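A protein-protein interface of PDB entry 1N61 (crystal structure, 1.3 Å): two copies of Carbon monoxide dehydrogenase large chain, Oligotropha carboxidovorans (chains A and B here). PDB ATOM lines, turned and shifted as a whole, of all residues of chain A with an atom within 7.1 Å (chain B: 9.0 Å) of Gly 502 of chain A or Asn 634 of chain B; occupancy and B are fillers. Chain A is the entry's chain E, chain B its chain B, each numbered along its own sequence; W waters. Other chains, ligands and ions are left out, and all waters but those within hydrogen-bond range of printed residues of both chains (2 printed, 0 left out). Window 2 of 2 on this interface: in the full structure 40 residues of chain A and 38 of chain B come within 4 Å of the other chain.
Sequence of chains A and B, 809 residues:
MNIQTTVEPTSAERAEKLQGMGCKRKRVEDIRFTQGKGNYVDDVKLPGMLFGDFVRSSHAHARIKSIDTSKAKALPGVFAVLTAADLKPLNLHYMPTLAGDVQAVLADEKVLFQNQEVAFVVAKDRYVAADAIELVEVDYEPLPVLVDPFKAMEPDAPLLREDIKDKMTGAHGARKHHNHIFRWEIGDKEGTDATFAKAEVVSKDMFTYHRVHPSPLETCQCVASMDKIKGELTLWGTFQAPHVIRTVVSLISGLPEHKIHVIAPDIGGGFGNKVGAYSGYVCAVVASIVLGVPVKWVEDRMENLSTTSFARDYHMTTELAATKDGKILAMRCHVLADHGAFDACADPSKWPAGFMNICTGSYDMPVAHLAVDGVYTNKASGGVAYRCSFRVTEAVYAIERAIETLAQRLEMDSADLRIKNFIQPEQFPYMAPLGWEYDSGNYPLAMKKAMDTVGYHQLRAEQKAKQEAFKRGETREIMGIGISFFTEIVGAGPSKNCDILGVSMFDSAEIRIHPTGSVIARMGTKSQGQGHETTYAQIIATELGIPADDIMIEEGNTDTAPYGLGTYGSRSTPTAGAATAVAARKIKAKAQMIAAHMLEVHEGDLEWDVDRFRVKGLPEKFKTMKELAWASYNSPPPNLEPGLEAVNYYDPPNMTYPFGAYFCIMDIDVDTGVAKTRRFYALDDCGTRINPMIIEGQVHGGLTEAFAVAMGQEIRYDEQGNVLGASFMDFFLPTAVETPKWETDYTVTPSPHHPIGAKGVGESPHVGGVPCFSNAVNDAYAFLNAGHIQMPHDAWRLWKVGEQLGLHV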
ATOM      1  N   SER A 349      -8.538  11.070 -25.391  1.00  0.00           N
ATOM      2  CA  SER A 349      -9.118   9.841 -25.911  1.00  0.00           C
ATOM      3  C   SER A 349      -9.571   8.865 -24.832  1.00  0.00           C
ATOM      4  O   SER A 349     -10.460   8.068 -25.084  1.00  0.00           O
ATOM      5  CB  SER A 349      -8.199   9.119 -26.918  1.00  0.00           C
ATOM      6  OG  SER A 349      -7.124   8.525 -26.244  1.00  0.00           O
ATOM      7  N   SER A 495       1.426  13.078 -20.343  1.00  0.00           N
ATOM      8  CA  SER A 495       1.431  12.078 -21.402  1.00  0.00           C
ATOM      9  C   SER A 495       0.903  10.716 -20.943  1.00  0.00           C
ATOM     10  O   SER A 495       0.442   9.920 -21.761  1.00  0.00           O
ATOM     11  CB  SER A 495       2.851  11.950 -21.960  1.00  0.00           C
ATOM     12  OG  SER A 495       3.785  11.596 -20.960  1.00  0.00           O
ATOM     13  N   CYS A 498      -3.224  11.663 -21.006  1.00  0.00           N
ATOM     14  CA  CYS A 498      -3.878  12.677 -21.867  1.00  0.00           C
ATOM     15  C   CYS A 498      -3.303  12.650 -23.271  1.00  0.00           C
ATOM     16  O   CYS A 498      -2.146  12.917 -23.496  1.00  0.00           O
ATOM     17  CB  CYS A 498      -3.690  14.085 -21.293  1.00  0.00           C
ATOM     18  SG  CYS A 498      -4.601  14.305 -19.748  1.00  0.00           S
ATOM     19  N   ASP A 499      -4.140  12.288 -24.234  1.00  0.00           N
ATOM     20  CA  ASP A 499      -3.756  12.281 -25.646  1.00  0.00           C
ATOM     21  C   ASP A 499      -4.980  12.641 -26.495  1.00  0.00           C
ATOM     22  O   ASP A 499      -6.090  12.389 -26.103  1.00  0.00           O
ATOM     23  CB  ASP A 499      -3.213  10.914 -26.046  1.00  0.00           C
ATOM     24  CG  ASP A 499      -4.289   9.868 -26.062  1.00  0.00           C
ATOM     25  OD1 ASP A 499      -4.526   9.257 -24.987  1.00  0.00           O
ATOM     26  OD2 ASP A 499      -4.928   9.608 -27.096  1.00  0.00           O
ATOM     27  N   ILE A 500      -4.740  13.248 -27.650  1.00  0.00           N
ATOM     28  CA  ILE A 500      -5.761  13.484 -28.661  1.00  0.00           C
ATOM     29  C   ILE A 500      -5.446  12.559 -29.819  1.00  0.00           C
ATOM     30  O   ILE A 500      -4.434  12.715 -30.501  1.00  0.00           O
ATOM     31  CB  ILE A 500      -5.751  14.942 -29.144  1.00  0.00           C
ATOM     32  CG1 ILE A 500      -6.079  15.904 -28.000  1.00  0.00           C
ATOM     33  CG2 ILE A 500      -6.690  15.104 -30.320  1.00  0.00           C
ATOM     34  CD1 ILE A 500      -7.556  15.884 -27.501  1.00  0.00           C
ATOM     35  N   LEU A 501      -6.303  11.565 -30.016  1.00  0.00           N
ATOM     36  CA  LEU A 501      -6.098  10.577 -31.051  1.00  0.00           C
ATOM     37  C   LEU A 501      -4.671  10.069 -31.100  1.00  0.00           C
ATOM     38  O   LEU A 501      -4.090   9.868 -32.188  1.00  0.00           O
ATOM     39  CB  LEU A 501      -6.488  11.161 -32.400  1.00  0.00           C
ATOM     40  CG  LEU A 501      -7.932  11.638 -32.489  1.00  0.00           C
ATOM     41  CD1 LEU A 501      -8.206  12.202 -33.889  1.00  0.00           C
ATOM     42  CD2 LEU A 501      -8.856  10.485 -32.168  1.00  0.00           C
ATOM     43  N   GLY A 502      -4.132   9.752 -29.931  1.00  0.00           N
ATOM     44  CA  GLY A 502      -2.834   9.122 -29.834  1.00  0.00           C
ATOM     45  C   GLY A 502      -1.636  10.063 -29.784  1.00  0.00           C
ATOM     46  O   GLY A 502      -0.544   9.644 -29.443  1.00  0.00           O
ATOM     47  N   VAL A 503      -1.885  11.346 -29.890  1.00  0.00           N
ATOM     48  CA  VAL A 503      -0.829  12.337 -29.721  1.00  0.00           C
ATOM     49  C   VAL A 503      -0.896  12.872 -28.303  1.00  0.00           C
ATOM     50  O   VAL A 503      -1.899  13.433 -27.892  1.00  0.00           O
ATOM     51  CB  VAL A 503      -0.922  13.461 -30.761  1.00  0.00           C
ATOM     52  CG1 VAL A 503       0.137  14.466 -30.509  1.00  0.00           C
ATOM     53  CG2 VAL A 503      -0.792  12.914 -32.156  1.00  0.00           C
ATOM     54  N   SER A 504       0.191  12.722 -27.562  1.00  0.00           N
ATOM     55  CA  SER A 504       0.213  13.172 -26.191  1.00  0.00           C
ATOM     56  C   SER A 504      -0.011  14.668 -26.075  1.00  0.00           C
ATOM     57  O   SER A 504       0.364  15.401 -26.985  1.00  0.00           O
ATOM     58  CB  SER A 504       1.587  12.867 -25.636  1.00  0.00           C
ATOM     59  OG  SER A 504       1.770  11.501 -25.693  1.00  0.00           O
ATOM     60  N   MET A 505      -0.711  15.101 -25.027  1.00  0.00           N
ATOM     61  CA  MET A 505      -1.150  16.485 -24.950  1.00  0.00           C
ATOM     62  C   MET A 505      -0.078  17.384 -24.306  1.00  0.00           C
ATOM     63  O   MET A 505      -0.316  18.083 -23.323  1.00  0.00           O
ATOM     64  CB  MET A 505      -2.483  16.528 -24.227  1.00  0.00           C
ATOM     65  CG  MET A 505      -3.569  15.863 -25.065  1.00  0.00           C
ATOM     66  SD  MET A 505      -5.168  15.942 -24.286  1.00  0.00           S
ATOM     67  CE  MET A 505      -5.549  17.631 -24.516  1.00  0.00           C
ATOM     68  N   PHE A 506       1.043  17.504 -25.016  1.00  0.00           N
ATOM     69  CA  PHE A 506       2.101  18.462 -24.717  1.00  0.00           C
ATOM     70  C   PHE A 506       1.753  19.768 -25.419  1.00  0.00           C
ATOM     71  O   PHE A 506       0.770  19.847 -26.164  1.00  0.00           O
ATOM     72  CB  PHE A 506       3.471  17.947 -25.155  1.00  0.00           C
ATOM     73  CG  PHE A 506       3.557  17.655 -26.622  1.00  0.00           C
ATOM     74  CD1 PHE A 506       3.816  18.677 -27.525  1.00  0.00           C
ATOM     75  CD2 PHE A 506       3.261  16.395 -27.124  1.00  0.00           C
ATOM     76  CE1 PHE A 506       3.730  18.484 -28.883  1.00  0.00           C
ATOM     77  CE2 PHE A 506       3.190  16.181 -28.491  1.00  0.00           C
ATOM     78  CZ  PHE A 506       3.412  17.224 -29.375  1.00  0.00           C
ATOM     79  N   PRO B 515       4.439  13.695 -37.017  1.00  0.00           N
ATOM     80  CA  PRO B 515       4.044  12.440 -36.337  1.00  0.00           C
ATOM     81  C   PRO B 515       3.962  11.253 -37.289  1.00  0.00           C
ATOM     82  O   PRO B 515       4.262  10.140 -36.856  1.00  0.00           O
ATOM     83  CB  PRO B 515       2.661  12.774 -35.761  1.00  0.00           C
ATOM     84  CG  PRO B 515       2.749  14.264 -35.516  1.00  0.00           C
ATOM     85  CD  PRO B 515       3.575  14.822 -36.688  1.00  0.00           C
ATOM     86  N   ILE B 594      14.879   6.575 -28.081  1.00  0.00           N
ATOM     87  CA  ILE B 594      13.489   6.154 -28.070  1.00  0.00           C
ATOM     88  C   ILE B 594      13.422   4.677 -28.384  1.00  0.00           C
ATOM     89  O   ILE B 594      12.702   3.918 -27.720  1.00  0.00           O
ATOM     90  CB  ILE B 594      12.659   6.955 -29.078  1.00  0.00           C
ATOM     91  CG1 ILE B 594      12.653   8.439 -28.713  1.00  0.00           C
ATOM     92  CG2 ILE B 594      11.281   6.410 -29.174  1.00  0.00           C
ATOM     93  CD1 ILE B 594      12.040   9.328 -29.809  1.00  0.00           C
ATOM     94  N   MET B 598      11.769   1.601 -26.089  1.00  0.00           N
ATOM     95  CA  MET B 598      10.699   0.776 -26.619  1.00  0.00           C
ATOM     96  C   MET B 598      11.077  -0.701 -26.692  1.00  0.00           C
ATOM     97  O   MET B 598      10.244  -1.567 -26.382  1.00  0.00           O
ATOM     98  CB  MET B 598      10.293   1.271 -28.002  1.00  0.00           C
ATOM     99  CG  MET B 598       9.636   2.600 -28.072  1.00  0.00           C
ATOM    100  SD  MET B 598       9.178   3.131 -29.758  1.00  0.00           S
ATOM    101  CE  MET B 598       7.730   2.271 -29.849  1.00  0.00           C
ATOM    102  N   GLU B 627       8.331   4.537 -37.168  1.00  0.00           N
ATOM    103  CA  GLU B 627       7.730   4.119 -35.920  1.00  0.00           C
ATOM    104  C   GLU B 627       8.236   5.009 -34.783  1.00  0.00           C
ATOM    105  O   GLU B 627       7.479   5.359 -33.861  1.00  0.00           O
ATOM    106  CB  GLU B 627       8.053   2.648 -35.638  1.00  0.00           C
ATOM    107  CG  GLU B 627       7.333   1.685 -36.552  1.00  0.00           C
ATOM    108  CD  GLU B 627       7.761   0.237 -36.414  1.00  0.00           C
ATOM    109  OE1 GLU B 627       6.890  -0.624 -36.635  1.00  0.00           O
ATOM    110  OE2 GLU B 627       8.940  -0.065 -36.167  1.00  0.00           O
ATOM    111  N   LEU B 628       9.501   5.383 -34.853  1.00  0.00           N
ATOM    112  CA  LEU B 628      10.083   6.169 -33.783  1.00  0.00           C
ATOM    113  C   LEU B 628       9.535   7.577 -33.790  1.00  0.00           C
ATOM    114  O   LEU B 628       9.354   8.218 -32.755  1.00  0.00           O
ATOM    115  CB  LEU B 628      11.613   6.149 -33.886  1.00  0.00           C
ATOM    116  CG  LEU B 628      12.164   4.752 -33.655  1.00  0.00           C
ATOM    117  CD1 LEU B 628      13.587   4.588 -34.099  1.00  0.00           C
ATOM    118  CD2 LEU B 628      11.988   4.302 -32.199  1.00  0.00           C
ATOM    119  N   ALA B 629       9.329   8.100 -34.992  1.00  0.00           N
ATOM    120  CA  ALA B 629       8.755   9.414 -35.129  1.00  0.00           C
ATOM    121  C   ALA B 629       7.360   9.421 -34.493  1.00  0.00           C
ATOM    122  O   ALA B 629       7.014  10.347 -33.770  1.00  0.00           O
ATOM    123  CB  ALA B 629       8.681   9.831 -36.601  1.00  0.00           C
ATOM    124  N   TRP B 630       6.518   8.438 -34.787  1.00  0.00           N
ATOM    125  CA  TRP B 630       5.200   8.404 -34.152  1.00  0.00           C
ATOM    126  C   TRP B 630       5.320   8.299 -32.630  1.00  0.00           C
ATOM    127  O   TRP B 630       4.683   9.012 -31.875  1.00  0.00           O
ATOM    128  CB  TRP B 630       4.410   7.239 -34.704  1.00  0.00           C
ATOM    129  CG  TRP B 630       3.078   7.054 -34.039  1.00  0.00           C
ATOM    130  CD1 TRP B 630       2.735   6.008 -33.227  1.00  0.00           C
ATOM    131  CD2 TRP B 630       2.015   7.999 -33.932  1.00  0.00           C
ATOM    132  NE1 TRP B 630       1.454   6.169 -32.759  1.00  0.00           N
ATOM    133  CE2 TRP B 630       1.007   7.405 -33.131  1.00  0.00           C
ATOM    134  CE3 TRP B 630       1.706   9.187 -34.595  1.00  0.00           C
ATOM    135  CZ2 TRP B 630      -0.224   7.997 -32.940  1.00  0.00           C
ATOM    136  CZ3 TRP B 630       0.565   9.819 -34.289  1.00  0.00           C
ATOM    137  CH2 TRP B 630      -0.435   9.194 -33.541  1.00  0.00           C
ATOM    138  N   ALA B 631       6.201   7.439 -32.183  1.00  0.00           N
ATOM    139  CA  ALA B 631       6.392   7.194 -30.762  1.00  0.00           C
ATOM    140  C   ALA B 631       6.819   8.493 -30.045  1.00  0.00           C
ATOM    141  O   ALA B 631       6.447   8.732 -28.890  1.00  0.00           O
ATOM    142  CB  ALA B 631       7.430   6.105 -30.575  1.00  0.00           C
ATOM    143  N   SER B 632       7.622   9.316 -30.715  1.00  0.00           N
ATOM    144  CA  SER B 632       8.093  10.548 -30.075  1.00  0.00           C
ATOM    145  C   SER B 632       6.925  11.474 -29.713  1.00  0.00           C
ATOM    146  O   SER B 632       7.070  12.324 -28.840  1.00  0.00           O
ATOM    147  CB  SER B 632       9.115  11.285 -30.956  1.00  0.00           C
ATOM    148  OG  SER B 632       8.453  11.974 -32.008  1.00  0.00           O
ATOM    149  N   TYR B 633       5.800  11.346 -30.418  1.00  0.00           N
ATOM    150  CA  TYR B 633       4.608  12.145 -30.160  1.00  0.00           C
ATOM    151  C   TYR B 633       3.609  11.360 -29.301  1.00  0.00           C
ATOM    152  O   TYR B 633       2.871  11.949 -28.497  1.00  0.00           O
ATOM    153  CB  TYR B 633       3.953  12.546 -31.486  1.00  0.00           C
ATOM    154  CG  TYR B 633       4.694  13.569 -32.307  1.00  0.00           C
ATOM    155  CD1 TYR B 633       5.593  13.204 -33.258  1.00  0.00           C
ATOM    156  CD2 TYR B 633       4.400  14.926 -32.184  1.00  0.00           C
ATOM    157  CE1 TYR B 633       6.292  14.147 -34.003  1.00  0.00           C
ATOM    158  CE2 TYR B 633       5.053  15.864 -32.931  1.00  0.00           C
ATOM    159  CZ  TYR B 633       5.992  15.476 -33.849  1.00  0.00           C
ATOM    160  OH  TYR B 633       6.576  16.401 -34.693  1.00  0.00           O
ATOM    161  N   ASN B 634       3.532  10.045 -29.491  1.00  0.00           N
ATOM    162  CA  ASN B 634       2.490   9.213 -28.899  1.00  0.00           C
ATOM    163  C   ASN B 634       2.874   8.735 -27.535  1.00  0.00           C
ATOM    164  O   ASN B 634       2.009   8.565 -26.694  1.00  0.00           O
ATOM    165  CB  ASN B 634       2.269   7.997 -29.794  1.00  0.00           C
ATOM    166  CG  ASN B 634       1.530   6.868 -29.099  1.00  0.00           C
ATOM    167  OD1 ASN B 634       2.075   5.783 -28.912  1.00  0.00           O
ATOM    168  ND2 ASN B 634       0.232   7.018 -29.002  1.00  0.00           N
ATOM    169  N   SER B 635       4.114   8.293 -27.393  1.00  0.00           N
ATOM    170  CA  SER B 635       4.593   7.777 -26.104  1.00  0.00           C
ATOM    171  C   SER B 635       6.015   8.211 -25.848  1.00  0.00           C
ATOM    172  O   SER B 635       6.944   7.408 -25.855  1.00  0.00           O
ATOM    173  CB  SER B 635       4.502   6.263 -25.990  1.00  0.00           C
ATOM    174  OG  SER B 635       4.569   5.919 -24.617  1.00  0.00           O
ATOM    175  N   PRO B 636       6.209   9.505 -25.625  1.00  0.00           N
ATOM    176  CA  PRO B 636       7.559  10.020 -25.331  1.00  0.00           C
ATOM    177  C   PRO B 636       8.180   9.338 -24.097  1.00  0.00           C
ATOM    178  O   PRO B 636       7.444   9.117 -23.168  1.00  0.00           O
ATOM    179  CB  PRO B 636       7.287  11.506 -25.025  1.00  0.00           C
ATOM    180  CG  PRO B 636       5.821  11.566 -24.739  1.00  0.00           C
ATOM    181  CD  PRO B 636       5.172  10.552 -25.582  1.00  0.00           C
ATOM    182  N   PRO B 637       9.363   8.755 -24.200  1.00  0.00           N
ATOM    183  CA  PRO B 637      10.006   8.175 -23.019  1.00  0.00           C
ATOM    184  C   PRO B 637      10.202   9.207 -21.894  1.00  0.00           C
ATOM    185  O   PRO B 637      10.315  10.387 -22.203  1.00  0.00           O
ATOM    186  CB  PRO B 637      11.352   7.685 -23.554  1.00  0.00           C
ATOM    187  CG  PRO B 637      11.216   7.662 -25.062  1.00  0.00           C
ATOM    188  CD  PRO B 637      10.233   8.721 -25.395  1.00  0.00           C
ATOM    189  N   GLU B 641      11.895  15.009 -24.192  1.00  0.00           N
ATOM    190  CA  GLU B 641      10.802  15.875 -24.629  1.00  0.00           C
ATOM    191  C   GLU B 641      10.048  15.121 -25.714  1.00  0.00           C
ATOM    192  O   GLU B 641      10.660  14.440 -26.535  1.00  0.00           O
ATOM    193  CB  GLU B 641      11.363  17.176 -25.199  1.00  0.00           C
ATOM    194  CG  GLU B 641      11.983  18.088 -24.147  1.00  0.00           C
ATOM    195  CD  GLU B 641      12.455  19.450 -24.628  1.00  0.00           C
ATOM    196  OE1 GLU B 641      11.890  19.958 -25.651  1.00  0.00           O
ATOM    197  OE2 GLU B 641      13.308  20.042 -23.899  1.00  0.00           O
ATOM    198  N   PRO B 642       8.767  15.435 -25.884  1.00  0.00           N
ATOM    199  CA  PRO B 642       8.045  14.943 -27.052  1.00  0.00           C
ATOM    200  C   PRO B 642       8.602  15.512 -28.324  1.00  0.00           C
ATOM    201  O   PRO B 642       9.331  16.521 -28.296  1.00  0.00           O
ATOM    202  CB  PRO B 642       6.620  15.424 -26.819  1.00  0.00           C
ATOM    203  CG  PRO B 642       6.534  15.605 -25.347  1.00  0.00           C
ATOM    204  CD  PRO B 642       7.891  16.069 -24.907  1.00  0.00           C
ATOM    205  N   GLY B 643       8.236  14.893 -29.427  1.00  0.00           N
ATOM    206  CA  GLY B 643       8.588  15.343 -30.752  1.00  0.00           C
ATOM    207  C   GLY B 643       9.961  14.872 -31.186  1.00  0.00           C
ATOM    208  O   GLY B 643      10.658  14.184 -30.457  1.00  0.00           O
HETATM  209  O   HOH W   1       2.563   7.542 -22.893  1.00  0.00           O
HETATM  210  O   HOH W   2       4.664   9.209 -22.468  1.00  0.00           O
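Of the 17 printed residues of chain B, 5 touch a printed residue of chain A. Of the 11 printed residues of chain A, 5 touch a printed residue of chain B. Printed residues of chain A that touch a printed residue of chain B: Leu 501, Gly 502, Val 503, Ser 504 and Phe 506. Hydrophobic or aromatic side chains of chain A that line the printed part of chain B: Val 503 and Phe 506. Among the printed residues, 10 pairs touch across the chains. Among the printed residues, no Asp or Glu carboxylate lies within 4 Å of a Lys or Arg side-chain nitrogen of the other chain.
No position is printed for both chains.
Water W2 lies within hydrogen-bond range of the backbone carbonyl oxygen of Pro 636 of chain B (2.9 Å) and the side-chain hydroxyl of Ser 495 of chain A (3.0 Å). Water W1 lies within hydrogen-bond range of the side-chain hydroxyl (OG) of Ser 635 of chain B (3.1 Å) and the backbone carbonyl oxygen (O) of Ser 495 of chain A (3.4 Å).
Printed residues of chain B within 4 Å of Gly 502 of chain A: Trp 630 (3.9 Å) and Asn 634 (2.8 Å). Of chain A, only Gly 502 (2.8 Å) and Ser 504 (3.1 Å) come within 4 Å of Asn 634 of chain B. Of the printed residues of chain B, Leu 501 of chain A touches Trp 630. Of the printed residues of chain A, Trp 630 of chain B touches Leu 501, Gly 502 and Val 503. Printed residues of chain B within 4 Å of Ser 504 of chain A: Tyr 633 (2.9 Å), Asn 634 (3.1 Å) and Pro 636 (3.5 Å). Of the printed residues of chain A, Pro 636 of chain B touches Ser 504 (3.5 Å). Ser 495 of chain A touches none of the printed residues of chain B. Cys 498 of chain A touches none of the printed residues of chain B. The nearest residue of chain B that does not touch Gly 502 of chain A is Tyr 633 of chain B (4.2 Å).
The backbone NH of Gly 502 of chain A is in hydrogen-bond range of the side-chain carboxylate of Asp 499 of chain A, at 2.9 Å.
The backbone carbonyl oxygen (O) of Tyr 633 of chain B lies within hydrogen-bond range of the backbone NH (N) of Ser 504 of chain A. ND2 of Asn 634 of chain B lies within hydrogen-bond range of O of Gly 502 of chain A (2.8 Å). The backbone carbonyl oxygen (O) of Asn 634 of chain B lies within hydrogen-bond range of the side-chain hydroxyl (OG) of Ser 504 of chain A (3.1 Å).
Among the printed residues, pairs that only touch across the chains: Leu 501 of chain A with Trp 630 of chain B (3.96 Å), Gly 502 of chain A with Trp 630 of chain B (3.9 Å), Val 503 of chain A with Trp 630 of chain B (3.99 Å), Val 503 of chain A with Tyr 633 of chain B (3.9 Å), Ser 504 of chain A with Pro 636 of chain B (3.5 Å), Phe 506 of chain A with Tyr 633 of chain B (3.8 Å) and Phe 506 of chain A with Pro 642 of chain B (3.5 Å).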
